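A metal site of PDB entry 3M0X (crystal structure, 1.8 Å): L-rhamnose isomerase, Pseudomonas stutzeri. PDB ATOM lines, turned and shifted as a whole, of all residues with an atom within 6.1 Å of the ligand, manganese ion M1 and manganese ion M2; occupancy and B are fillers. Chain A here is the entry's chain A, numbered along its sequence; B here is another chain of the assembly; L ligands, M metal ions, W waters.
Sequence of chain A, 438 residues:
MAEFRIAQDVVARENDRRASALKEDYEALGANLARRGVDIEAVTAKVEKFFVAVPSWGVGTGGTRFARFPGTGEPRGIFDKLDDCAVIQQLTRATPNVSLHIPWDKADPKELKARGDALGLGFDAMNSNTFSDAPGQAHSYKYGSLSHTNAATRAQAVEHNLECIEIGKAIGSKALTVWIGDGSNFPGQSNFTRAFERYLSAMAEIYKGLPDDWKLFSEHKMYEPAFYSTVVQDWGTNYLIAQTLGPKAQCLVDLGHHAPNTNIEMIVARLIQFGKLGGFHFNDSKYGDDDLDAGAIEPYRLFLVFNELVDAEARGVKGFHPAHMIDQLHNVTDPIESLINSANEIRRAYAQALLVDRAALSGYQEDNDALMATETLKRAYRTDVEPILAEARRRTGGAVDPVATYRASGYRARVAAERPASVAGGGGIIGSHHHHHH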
ATOM      1  N   TRP A  57      -1.534  10.634   1.909  1.00  0.00           N
ATOM      2  CA  TRP A  57      -0.722   9.614   2.578  1.00  0.00           C
ATOM      3  C   TRP A  57       0.466  10.183   3.341  1.00  0.00           C
ATOM      4  O   TRP A  57       1.200   9.439   4.004  1.00  0.00           O
ATOM      5  CB  TRP A  57      -0.260   8.576   1.550  1.00  0.00           C
ATOM      6  CG  TRP A  57       0.627   9.123   0.478  1.00  0.00           C
ATOM      7  CD1 TRP A  57       1.987   9.212   0.508  1.00  0.00           C
ATOM      8  CD2 TRP A  57       0.215   9.648  -0.788  1.00  0.00           C
ATOM      9  NE1 TRP A  57       2.453   9.743  -0.670  1.00  0.00           N
ATOM     10  CE2 TRP A  57       1.387  10.024  -1.480  1.00  0.00           C
ATOM     11  CE3 TRP A  57      -1.026   9.831  -1.402  1.00  0.00           C
ATOM     12  CZ2 TRP A  57       1.361  10.580  -2.765  1.00  0.00           C
ATOM     13  CZ3 TRP A  57      -1.053  10.386  -2.687  1.00  0.00           C
ATOM     14  CH2 TRP A  57       0.130  10.748  -3.347  1.00  0.00           C
ATOM     15  N   HIS A 101      -5.260   8.704  -2.855  1.00  0.00           N
ATOM     16  CA  HIS A 101      -4.674   7.415  -3.209  1.00  0.00           C
ATOM     17  C   HIS A 101      -5.748   6.361  -2.963  1.00  0.00           C
ATOM     18  O   HIS A 101      -6.300   6.259  -1.865  1.00  0.00           O
ATOM     19  CB  HIS A 101      -3.431   7.130  -2.366  1.00  0.00           C
ATOM     20  CG  HIS A 101      -2.334   6.466  -3.128  1.00  0.00           C
ATOM     21  ND1 HIS A 101      -2.430   5.180  -3.609  1.00  0.00           N
ATOM     22  CD2 HIS A 101      -1.108   6.910  -3.501  1.00  0.00           C
ATOM     23  CE1 HIS A 101      -1.312   4.863  -4.251  1.00  0.00           C
ATOM     24  NE2 HIS A 101      -0.491   5.904  -4.198  1.00  0.00           N
ATOM     25  N   TRP A 104      -6.557   3.403  -0.467  1.00  0.00           N
ATOM     26  CA  TRP A 104      -6.339   3.939   0.880  1.00  0.00           C
ATOM     27  C   TRP A 104      -7.397   4.966   1.254  1.00  0.00           C
ATOM     28  O   TRP A 104      -7.949   4.911   2.358  1.00  0.00           O
ATOM     29  CB  TRP A 104      -4.960   4.587   1.018  1.00  0.00           C
ATOM     30  CG  TRP A 104      -3.794   3.663   0.848  1.00  0.00           C
ATOM     31  CD1 TRP A 104      -3.787   2.305   1.003  1.00  0.00           C
ATOM     32  CD2 TRP A 104      -2.450   4.042   0.504  1.00  0.00           C
ATOM     33  NE1 TRP A 104      -2.521   1.815   0.768  1.00  0.00           N
ATOM     34  CE2 TRP A 104      -1.683   2.853   0.455  1.00  0.00           C
ATOM     35  CE3 TRP A 104      -1.829   5.262   0.218  1.00  0.00           C
ATOM     36  CZ2 TRP A 104      -0.316   2.850   0.153  1.00  0.00           C
ATOM     37  CZ3 TRP A 104      -0.475   5.261  -0.083  1.00  0.00           C
ATOM     38  CH2 TRP A 104       0.268   4.066  -0.115  1.00  0.00           C
ATOM     39  N   ASN A 127      -4.357   8.762  -7.613  1.00  0.00           N
ATOM     40  CA  ASN A 127      -3.238   7.823  -7.602  1.00  0.00           C
ATOM     41  C   ASN A 127      -3.797   6.430  -7.413  1.00  0.00           C
ATOM     42  O   ASN A 127      -4.532   6.176  -6.455  1.00  0.00           O
ATOM     43  CB  ASN A 127      -2.300   8.149  -6.443  1.00  0.00           C
ATOM     44  CG  ASN A 127      -1.662   9.510  -6.590  1.00  0.00           C
ATOM     45  OD1 ASN A 127      -0.596   9.645  -7.192  1.00  0.00           O
ATOM     46  ND2 ASN A 127      -2.306  10.529  -6.048  1.00  0.00           N
ATOM     47  N   SER A 128      -3.454   5.530  -8.335  1.00  0.00           N
ATOM     48  CA  SER A 128      -3.912   4.150  -8.256  1.00  0.00           C
ATOM     49  C   SER A 128      -2.933   3.325  -7.436  1.00  0.00           C
ATOM     50  O   SER A 128      -1.788   3.732  -7.234  1.00  0.00           O
ATOM     51  CB  SER A 128      -4.028   3.559  -9.669  1.00  0.00           C
ATOM     52  OG  SER A 128      -2.800   3.649 -10.371  1.00  0.00           O
ATOM     53  N   PHE A 131       0.371  -2.017  -6.321  1.00  0.00           N
ATOM     54  CA  PHE A 131       1.663  -2.446  -5.794  1.00  0.00           C
ATOM     55  C   PHE A 131       1.467  -3.121  -4.433  1.00  0.00           C
ATOM     56  O   PHE A 131       2.417  -3.381  -3.698  1.00  0.00           O
ATOM     57  CB  PHE A 131       2.622  -1.245  -5.691  1.00  0.00           C
ATOM     58  CG  PHE A 131       2.061  -0.058  -4.954  1.00  0.00           C
ATOM     59  CD1 PHE A 131       1.963  -0.057  -3.563  1.00  0.00           C
ATOM     60  CD2 PHE A 131       1.617   1.057  -5.663  1.00  0.00           C
ATOM     61  CE1 PHE A 131       1.441   1.043  -2.895  1.00  0.00           C
ATOM     62  CE2 PHE A 131       1.088   2.163  -4.990  1.00  0.00           C
ATOM     63  CZ  PHE A 131       1.003   2.153  -3.609  1.00  0.00           C
ATOM     64  N   THR A 177      -2.410   9.461 -11.825  1.00  0.00           N
ATOM     65  CA  THR A 177      -0.989   9.172 -11.770  1.00  0.00           C
ATOM     66  C   THR A 177      -0.842   7.681 -11.534  1.00  0.00           C
ATOM     67  O   THR A 177      -1.486   7.124 -10.643  1.00  0.00           O
ATOM     68  CB  THR A 177      -0.306   9.916 -10.635  1.00  0.00           C
ATOM     69  OG1 THR A 177      -0.394  11.329 -10.881  1.00  0.00           O
ATOM     70  CG2 THR A 177       1.159   9.515 -10.528  1.00  0.00           C
ATOM     71  N   TRP A 179       1.849   4.771 -10.686  1.00  0.00           N
ATOM     72  CA  TRP A 179       3.168   4.307 -10.265  1.00  0.00           C
ATOM     73  C   TRP A 179       2.949   2.868  -9.817  1.00  0.00           C
ATOM     74  O   TRP A 179       2.066   2.589  -9.005  1.00  0.00           O
ATOM     75  CB  TRP A 179       3.726   5.088  -9.073  1.00  0.00           C
ATOM     76  CG  TRP A 179       5.000   4.446  -8.599  1.00  0.00           C
ATOM     77  CD1 TRP A 179       6.193   4.414  -9.262  1.00  0.00           C
ATOM     78  CD2 TRP A 179       5.157   3.582  -7.465  1.00  0.00           C
ATOM     79  NE1 TRP A 179       7.077   3.571  -8.628  1.00  0.00           N
ATOM     80  CE2 TRP A 179       6.467   3.058  -7.520  1.00  0.00           C
ATOM     81  CE3 TRP A 179       4.311   3.200  -6.416  1.00  0.00           C
ATOM     82  CZ2 TRP A 179       6.948   2.163  -6.555  1.00  0.00           C
ATOM     83  CZ3 TRP A 179       4.795   2.312  -5.458  1.00  0.00           C
ATOM     84  CH2 TRP A 179       6.106   1.794  -5.537  1.00  0.00           C
ATOM     85  N   GLU A 219       4.811   7.433 -13.670  1.00  0.00           N
ATOM     86  CA  GLU A 219       5.923   7.817 -12.824  1.00  0.00           C
ATOM     87  C   GLU A 219       7.040   6.769 -12.827  1.00  0.00           C
ATOM     88  O   GLU A 219       6.827   5.621 -12.437  1.00  0.00           O
ATOM     89  CB  GLU A 219       5.400   8.035 -11.397  1.00  0.00           C
ATOM     90  CG  GLU A 219       6.445   8.369 -10.353  1.00  0.00           C
ATOM     91  CD  GLU A 219       5.840   8.647  -8.983  1.00  0.00           C
ATOM     92  OE1 GLU A 219       4.653   8.315  -8.776  1.00  0.00           O
ATOM     93  OE2 GLU A 219       6.553   9.187  -8.115  1.00  0.00           O
ATOM     94  N   LYS A 221      10.787   5.077 -11.747  1.00  0.00           N
ATOM     95  CA  LYS A 221      11.517   4.878 -10.496  1.00  0.00           C
ATOM     96  C   LYS A 221      12.595   3.830 -10.756  1.00  0.00           C
ATOM     97  O   LYS A 221      12.300   2.735 -11.239  1.00  0.00           O
ATOM     98  CB  LYS A 221      10.555   4.404  -9.407  1.00  0.00           C
ATOM     99  CG  LYS A 221      11.157   4.437  -8.010  1.00  0.00           C
ATOM    100  CD  LYS A 221      10.172   3.940  -6.966  1.00  0.00           C
ATOM    101  CE  LYS A 221      10.733   4.127  -5.562  1.00  0.00           C
ATOM    102  NZ  LYS A 221       9.798   3.578  -4.532  1.00  0.00           N
ATOM    103  N   GLU A 224      13.020  -0.291  -6.156  1.00  0.00           N
ATOM    104  CA  GLU A 224      12.158  -0.374  -4.957  1.00  0.00           C
ATOM    105  C   GLU A 224      10.692  -0.189  -5.336  1.00  0.00           C
ATOM    106  O   GLU A 224      10.272   0.889  -5.742  1.00  0.00           O
ATOM    107  CB  GLU A 224      12.525   0.659  -3.892  1.00  0.00           C
ATOM    108  CG  GLU A 224      11.686   0.473  -2.620  1.00  0.00           C
ATOM    109  CD  GLU A 224      11.778   1.646  -1.657  1.00  0.00           C
ATOM    110  OE1 GLU A 224      11.896   2.799  -2.119  1.00  0.00           O
ATOM    111  OE2 GLU A 224      11.701   1.407  -0.441  1.00  0.00           O
ATOM    112  N   LEU A 252       5.686  11.918 -15.113  1.00  0.00           N
ATOM    113  CA  LEU A 252       5.743  12.554 -13.814  1.00  0.00           C
ATOM    114  C   LEU A 252       7.128  12.275 -13.242  1.00  0.00           C
ATOM    115  O   LEU A 252       7.583  11.130 -13.222  1.00  0.00           O
ATOM    116  CB  LEU A 252       4.657  12.025 -12.883  1.00  0.00           C
ATOM    117  CG  LEU A 252       4.642  12.762 -11.535  1.00  0.00           C
ATOM    118  CD1 LEU A 252       3.214  13.128 -11.158  1.00  0.00           C
ATOM    119  CD2 LEU A 252       5.295  11.893 -10.477  1.00  0.00           C
ATOM    120  N   ASP A 254       9.489  12.308 -10.003  1.00  0.00           N
ATOM    121  CA  ASP A 254       9.554  12.313  -8.545  1.00  0.00           C
ATOM    122  C   ASP A 254      11.046  12.488  -8.279  1.00  0.00           C
ATOM    123  O   ASP A 254      11.847  11.645  -8.662  1.00  0.00           O
ATOM    124  CB  ASP A 254       9.065  10.972  -7.977  1.00  0.00           C
ATOM    125  CG  ASP A 254       9.059  10.951  -6.458  1.00  0.00           C
ATOM    126  OD1 ASP A 254      10.082  11.296  -5.848  1.00  0.00           O
ATOM    127  OD2 ASP A 254       8.019  10.572  -5.874  1.00  0.00           O
ATOM    128  N   HIS A 257      13.551   9.537  -7.278  1.00  0.00           N
ATOM    129  CA  HIS A 257      13.518   8.293  -8.055  1.00  0.00           C
ATOM    130  C   HIS A 257      14.626   8.120  -9.090  1.00  0.00           C
ATOM    131  O   HIS A 257      14.455   7.397 -10.066  1.00  0.00           O
ATOM    132  CB  HIS A 257      12.169   8.176  -8.757  1.00  0.00           C
ATOM    133  CG  HIS A 257      11.014   7.933  -7.833  1.00  0.00           C
ATOM    134  ND1 HIS A 257       9.763   7.591  -8.297  1.00  0.00           N
ATOM    135  CD2 HIS A 257      10.935   7.952  -6.479  1.00  0.00           C
ATOM    136  CE1 HIS A 257       8.956   7.405  -7.269  1.00  0.00           C
ATOM    137  NE2 HIS A 257       9.637   7.624  -6.159  1.00  0.00           N
ATOM    138  N   HIS A 281       6.707  15.354  -8.318  1.00  0.00           N
ATOM    139  CA  HIS A 281       6.472  14.789  -6.996  1.00  0.00           C
ATOM    140  C   HIS A 281       7.665  15.335  -6.241  1.00  0.00           C
ATOM    141  O   HIS A 281       8.794  14.863  -6.412  1.00  0.00           O
ATOM    142  CB  HIS A 281       6.488  13.257  -7.008  1.00  0.00           C
ATOM    143  CG  HIS A 281       5.128  12.645  -7.105  1.00  0.00           C
ATOM    144  ND1 HIS A 281       4.899  11.302  -6.910  1.00  0.00           N
ATOM    145  CD2 HIS A 281       3.923  13.198  -7.378  1.00  0.00           C
ATOM    146  CE1 HIS A 281       3.605  11.051  -7.067  1.00  0.00           C
ATOM    147  NE2 HIS A 281       2.994  12.180  -7.356  1.00  0.00           N
ATOM    148  N   ASN A 283      10.101  16.287  -3.031  1.00  0.00           N
ATOM    149  CA  ASN A 283      10.617  15.729  -1.792  1.00  0.00           C
ATOM    150  C   ASN A 283      12.122  15.887  -1.880  1.00  0.00           C
ATOM    151  O   ASN A 283      12.640  16.339  -2.894  1.00  0.00           O
ATOM    152  CB  ASN A 283      10.246  14.239  -1.650  1.00  0.00           C
ATOM    153  CG  ASN A 283      10.615  13.418  -2.879  1.00  0.00           C
ATOM    154  OD1 ASN A 283      11.784  13.354  -3.287  1.00  0.00           O
ATOM    155  ND2 ASN A 283       9.617  12.786  -3.478  1.00  0.00           N
ATOM    156  N   ASP A 289      15.189   6.703  -2.342  1.00  0.00           N
ATOM    157  CA  ASP A 289      13.908   7.416  -2.418  1.00  0.00           C
ATOM    158  C   ASP A 289      13.515   7.695  -0.973  1.00  0.00           C
ATOM    159  O   ASP A 289      12.534   7.167  -0.461  1.00  0.00           O
ATOM    160  CB  ASP A 289      12.855   6.541  -3.124  1.00  0.00           C
ATOM    161  CG  ASP A 289      11.526   7.248  -3.276  1.00  0.00           C
ATOM    162  OD1 ASP A 289      11.537   8.504  -3.388  1.00  0.00           O
ATOM    163  OD2 ASP A 289      10.481   6.569  -3.304  1.00  0.00           O
ATOM    164  N   ASP A 291      12.187  10.228   0.508  1.00  0.00           N
ATOM    165  CA  ASP A 291      10.926  10.927   0.743  1.00  0.00           C
ATOM    166  C   ASP A 291      10.974  11.921   1.905  1.00  0.00           C
ATOM    167  O   ASP A 291      10.041  12.002   2.689  1.00  0.00           O
ATOM    168  CB  ASP A 291       9.808   9.908   0.989  1.00  0.00           C
ATOM    169  CG  ASP A 291       9.357   9.241  -0.281  1.00  0.00           C
ATOM    170  OD1 ASP A 291       9.167   9.975  -1.280  1.00  0.00           O
ATOM    171  OD2 ASP A 291       9.183   8.004  -0.286  1.00  0.00           O
ATOM    172  N   ASP A 327       5.299  14.572  -2.508  1.00  0.00           N
ATOM    173  CA  ASP A 327       5.189  13.139  -2.251  1.00  0.00           C
ATOM    174  C   ASP A 327       6.259  12.853  -1.224  1.00  0.00           C
ATOM    175  O   ASP A 327       7.420  12.620  -1.562  1.00  0.00           O
ATOM    176  CB  ASP A 327       5.440  12.285  -3.496  1.00  0.00           C
ATOM    177  CG  ASP A 327       5.290  10.789  -3.196  1.00  0.00           C
ATOM    178  OD1 ASP A 327       4.949  10.455  -2.049  1.00  0.00           O
ATOM    179  OD2 ASP A 327       5.507   9.958  -4.101  1.00  0.00           O
ATOM    180  N   ARG B  65       8.576  -1.679   2.266  1.00  0.00           N
ATOM    181  CA  ARG B  65       7.706  -0.734   2.948  1.00  0.00           C
ATOM    182  C   ARG B  65       6.399  -0.559   2.194  1.00  0.00           C
ATOM    183  O   ARG B  65       5.425   0.004   2.729  1.00  0.00           O
ATOM    184  CB  ARG B  65       8.388   0.629   3.104  1.00  0.00           C
ATOM    185  CG  ARG B  65       8.752   1.292   1.795  1.00  0.00           C
ATOM    186  CD  ARG B  65       9.161   2.756   2.001  1.00  0.00           C
ATOM    187  NE  ARG B  65       9.791   3.275   0.788  1.00  0.00           N
ATOM    188  CZ  ARG B  65       9.810   4.559   0.427  1.00  0.00           C
ATOM    189  NH1 ARG B  65       9.221   5.484   1.176  1.00  0.00           N
ATOM    190  NH2 ARG B  65      10.417   4.905  -0.710  1.00  0.00           N
ATOM    191  N   PHE B  66       6.355  -1.050   0.961  1.00  0.00           N
ATOM    192  CA  PHE B  66       5.157  -0.929   0.130  1.00  0.00           C
ATOM    193  C   PHE B  66       4.172  -2.073   0.315  1.00  0.00           C
ATOM    194  O   PHE B  66       2.966  -1.866   0.294  1.00  0.00           O
ATOM    195  CB  PHE B  66       5.554  -0.827  -1.339  1.00  0.00           C
ATOM    196  CG  PHE B  66       6.183   0.470  -1.687  1.00  0.00           C
ATOM    197  CD1 PHE B  66       5.410   1.631  -1.757  1.00  0.00           C
ATOM    198  CD2 PHE B  66       7.555   0.569  -1.880  1.00  0.00           C
ATOM    199  CE1 PHE B  66       5.988   2.853  -2.020  1.00  0.00           C
ATOM    200  CE2 PHE B  66       8.154   1.792  -2.138  1.00  0.00           C
ATOM    201  CZ  PHE B  66       7.364   2.939  -2.211  1.00  0.00           C
HETATM  202  C1  LIG L   1       6.679   5.365  -4.894  1.00  0.00           C
HETATM  203  O1  LIG L   1       8.051   5.483  -4.553  1.00  0.00           O
HETATM  204  C2  LIG L   1       6.099   6.733  -5.204  1.00  0.00           C
HETATM  205  O2  LIG L   1       6.811   7.736  -5.229  1.00  0.00           O
HETATM  206  C3  LIG L   1       4.673   6.812  -5.731  1.00  0.00           C
HETATM  207  O3  LIG L   1       4.377   8.140  -6.111  1.00  0.00           O
HETATM  208  C4  LIG L   1       3.682   6.333  -4.654  1.00  0.00           C
HETATM  209  O4  LIG L   1       2.395   6.191  -5.223  1.00  0.00           O
HETATM  210  C5  LIG L   1       3.618   7.303  -3.468  1.00  0.00           C
HETATM  211  O5  LIG L   1       4.932   7.549  -2.989  1.00  0.00           O
HETATM  212  C6  LIG L   1       2.782   6.684  -2.344  1.00  0.00           C
HETATM  213  O6  LIG L   1       3.479   5.590  -1.778  1.00  0.00           O
HETATM  214 MN    MN M   1       6.050   9.701  -6.094  1.00  0.00          MN
HETATM  215 MN    MN M   2       8.728   7.208  -4.307  1.00  0.00          MN
HETATM  216  O   HOH W   1       1.386   7.620  -7.411  1.00  0.00           O
HETATM  217  O   HOH W   2       9.104   9.082  -3.676  1.00  0.00           O
HETATM  218  O   HOH W   3       7.721   6.957  -2.376  1.00  0.00           O
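O1 of the ligand is bound to manganese ion M2 (1.9 Å). Manganese ion M2 is bound by water W2, at 2.0 Å. A ring nitrogen (NE2) of His 257 binds manganese ion M2, 2.1 Å away. OD2 of Asp 289 is bound to manganese ion M2, 2.1 Å away. Manganese ion M2 is bound by O2 of the ligand (2.2 Å). Water W3 binds manganese ion M2, at 2.2 Å.
Manganese ion M1 is bound by the side-chain carboxylate of Asp 327 (2.1 Å), a ring nitrogen (ND1) of His 281 (2.1 Å), the side-chain carboxylate of Glu 219 (2.1 Å), the side-chain carboxylate of Asp 254 (2.2 Å), an oxygen (O2) of the ligand (2.3 Å) and an oxygen (O3) of the ligand (2.3 Å).
Merely in contact with the ligand: Trp 57 (3.5 Å), Trp 104 (3.9 Å), Trp 179 (3.5 Å) and Phe 66 of chain B (3.5 Å). Hydrophobic or aromatic side chains within 4 Å of the ligand: Trp 57, His 101, Trp 104, Trp 179, His 257, His 281 and Phe 66 of chain B. Of the 21 residues printed, 12 come within 4 Å of the ligand.
The side-chain amino group of Lys 221 sits close to an oxygen (O1) of the ligand (2.6 Å). NE2 of His 101 lies within hydrogen-bond range of O4 of the ligand (3.1 Å).
NE1 of Trp 57 is in hydrogen-bond range of OD1 of Asp 327 (2.9 Å). The backbone carbonyl oxygen (O) of Asp 327 lies within hydrogen-bond range of the side-chain amide nitrogen (ND2) of Asn 283, 2.9 Å away. NZ of Lys 221 lies close to OD2 of Asp 289 (3.3 Å). The backbone carbonyl oxygen (O) of Asp 289 is in hydrogen-bond range of the guanidinium group (NH2) of Arg 65 of chain B, 3.1 Å away. The side-chain amide nitrogen (ND2) of Asn 283 sits at hydrogen-bond distance from the side-chain carboxylate (OD1) of Asp 254 (2.8 Å). The side-chain amino group (NZ) of Lys 221 is in salt-bridge range of the side-chain carboxylate (OE1) of Glu 224, 3.3 Å away.
NZ of Lys 221 touches manganese ion M2 (3.8 Å). Four residues have an atom within 4 Å of manganese ion M2: Lys 221, Asp 254, His 257 and Asp 289. The nearest printed residue that does not touch manganese ion M2 is Asp 291 (4.1 Å).
Five residues have an atom within 4 Å of manganese ion M1: Glu 219, Asp 254, His 257, His 281 and Asp 327. The nearest printed residue that does not touch manganese ion M1 is Leu 252 (5.0 Å).
Water W3 lies within hydrogen-bond range of OD2 of Asp 291 (2.8 Å) and O5 of the ligand (2.9 Å). Water W1 lies within hydrogen-bond range of O4 of the ligand (2.8 Å) and OD1 of Asn 127 (2.8 Å).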
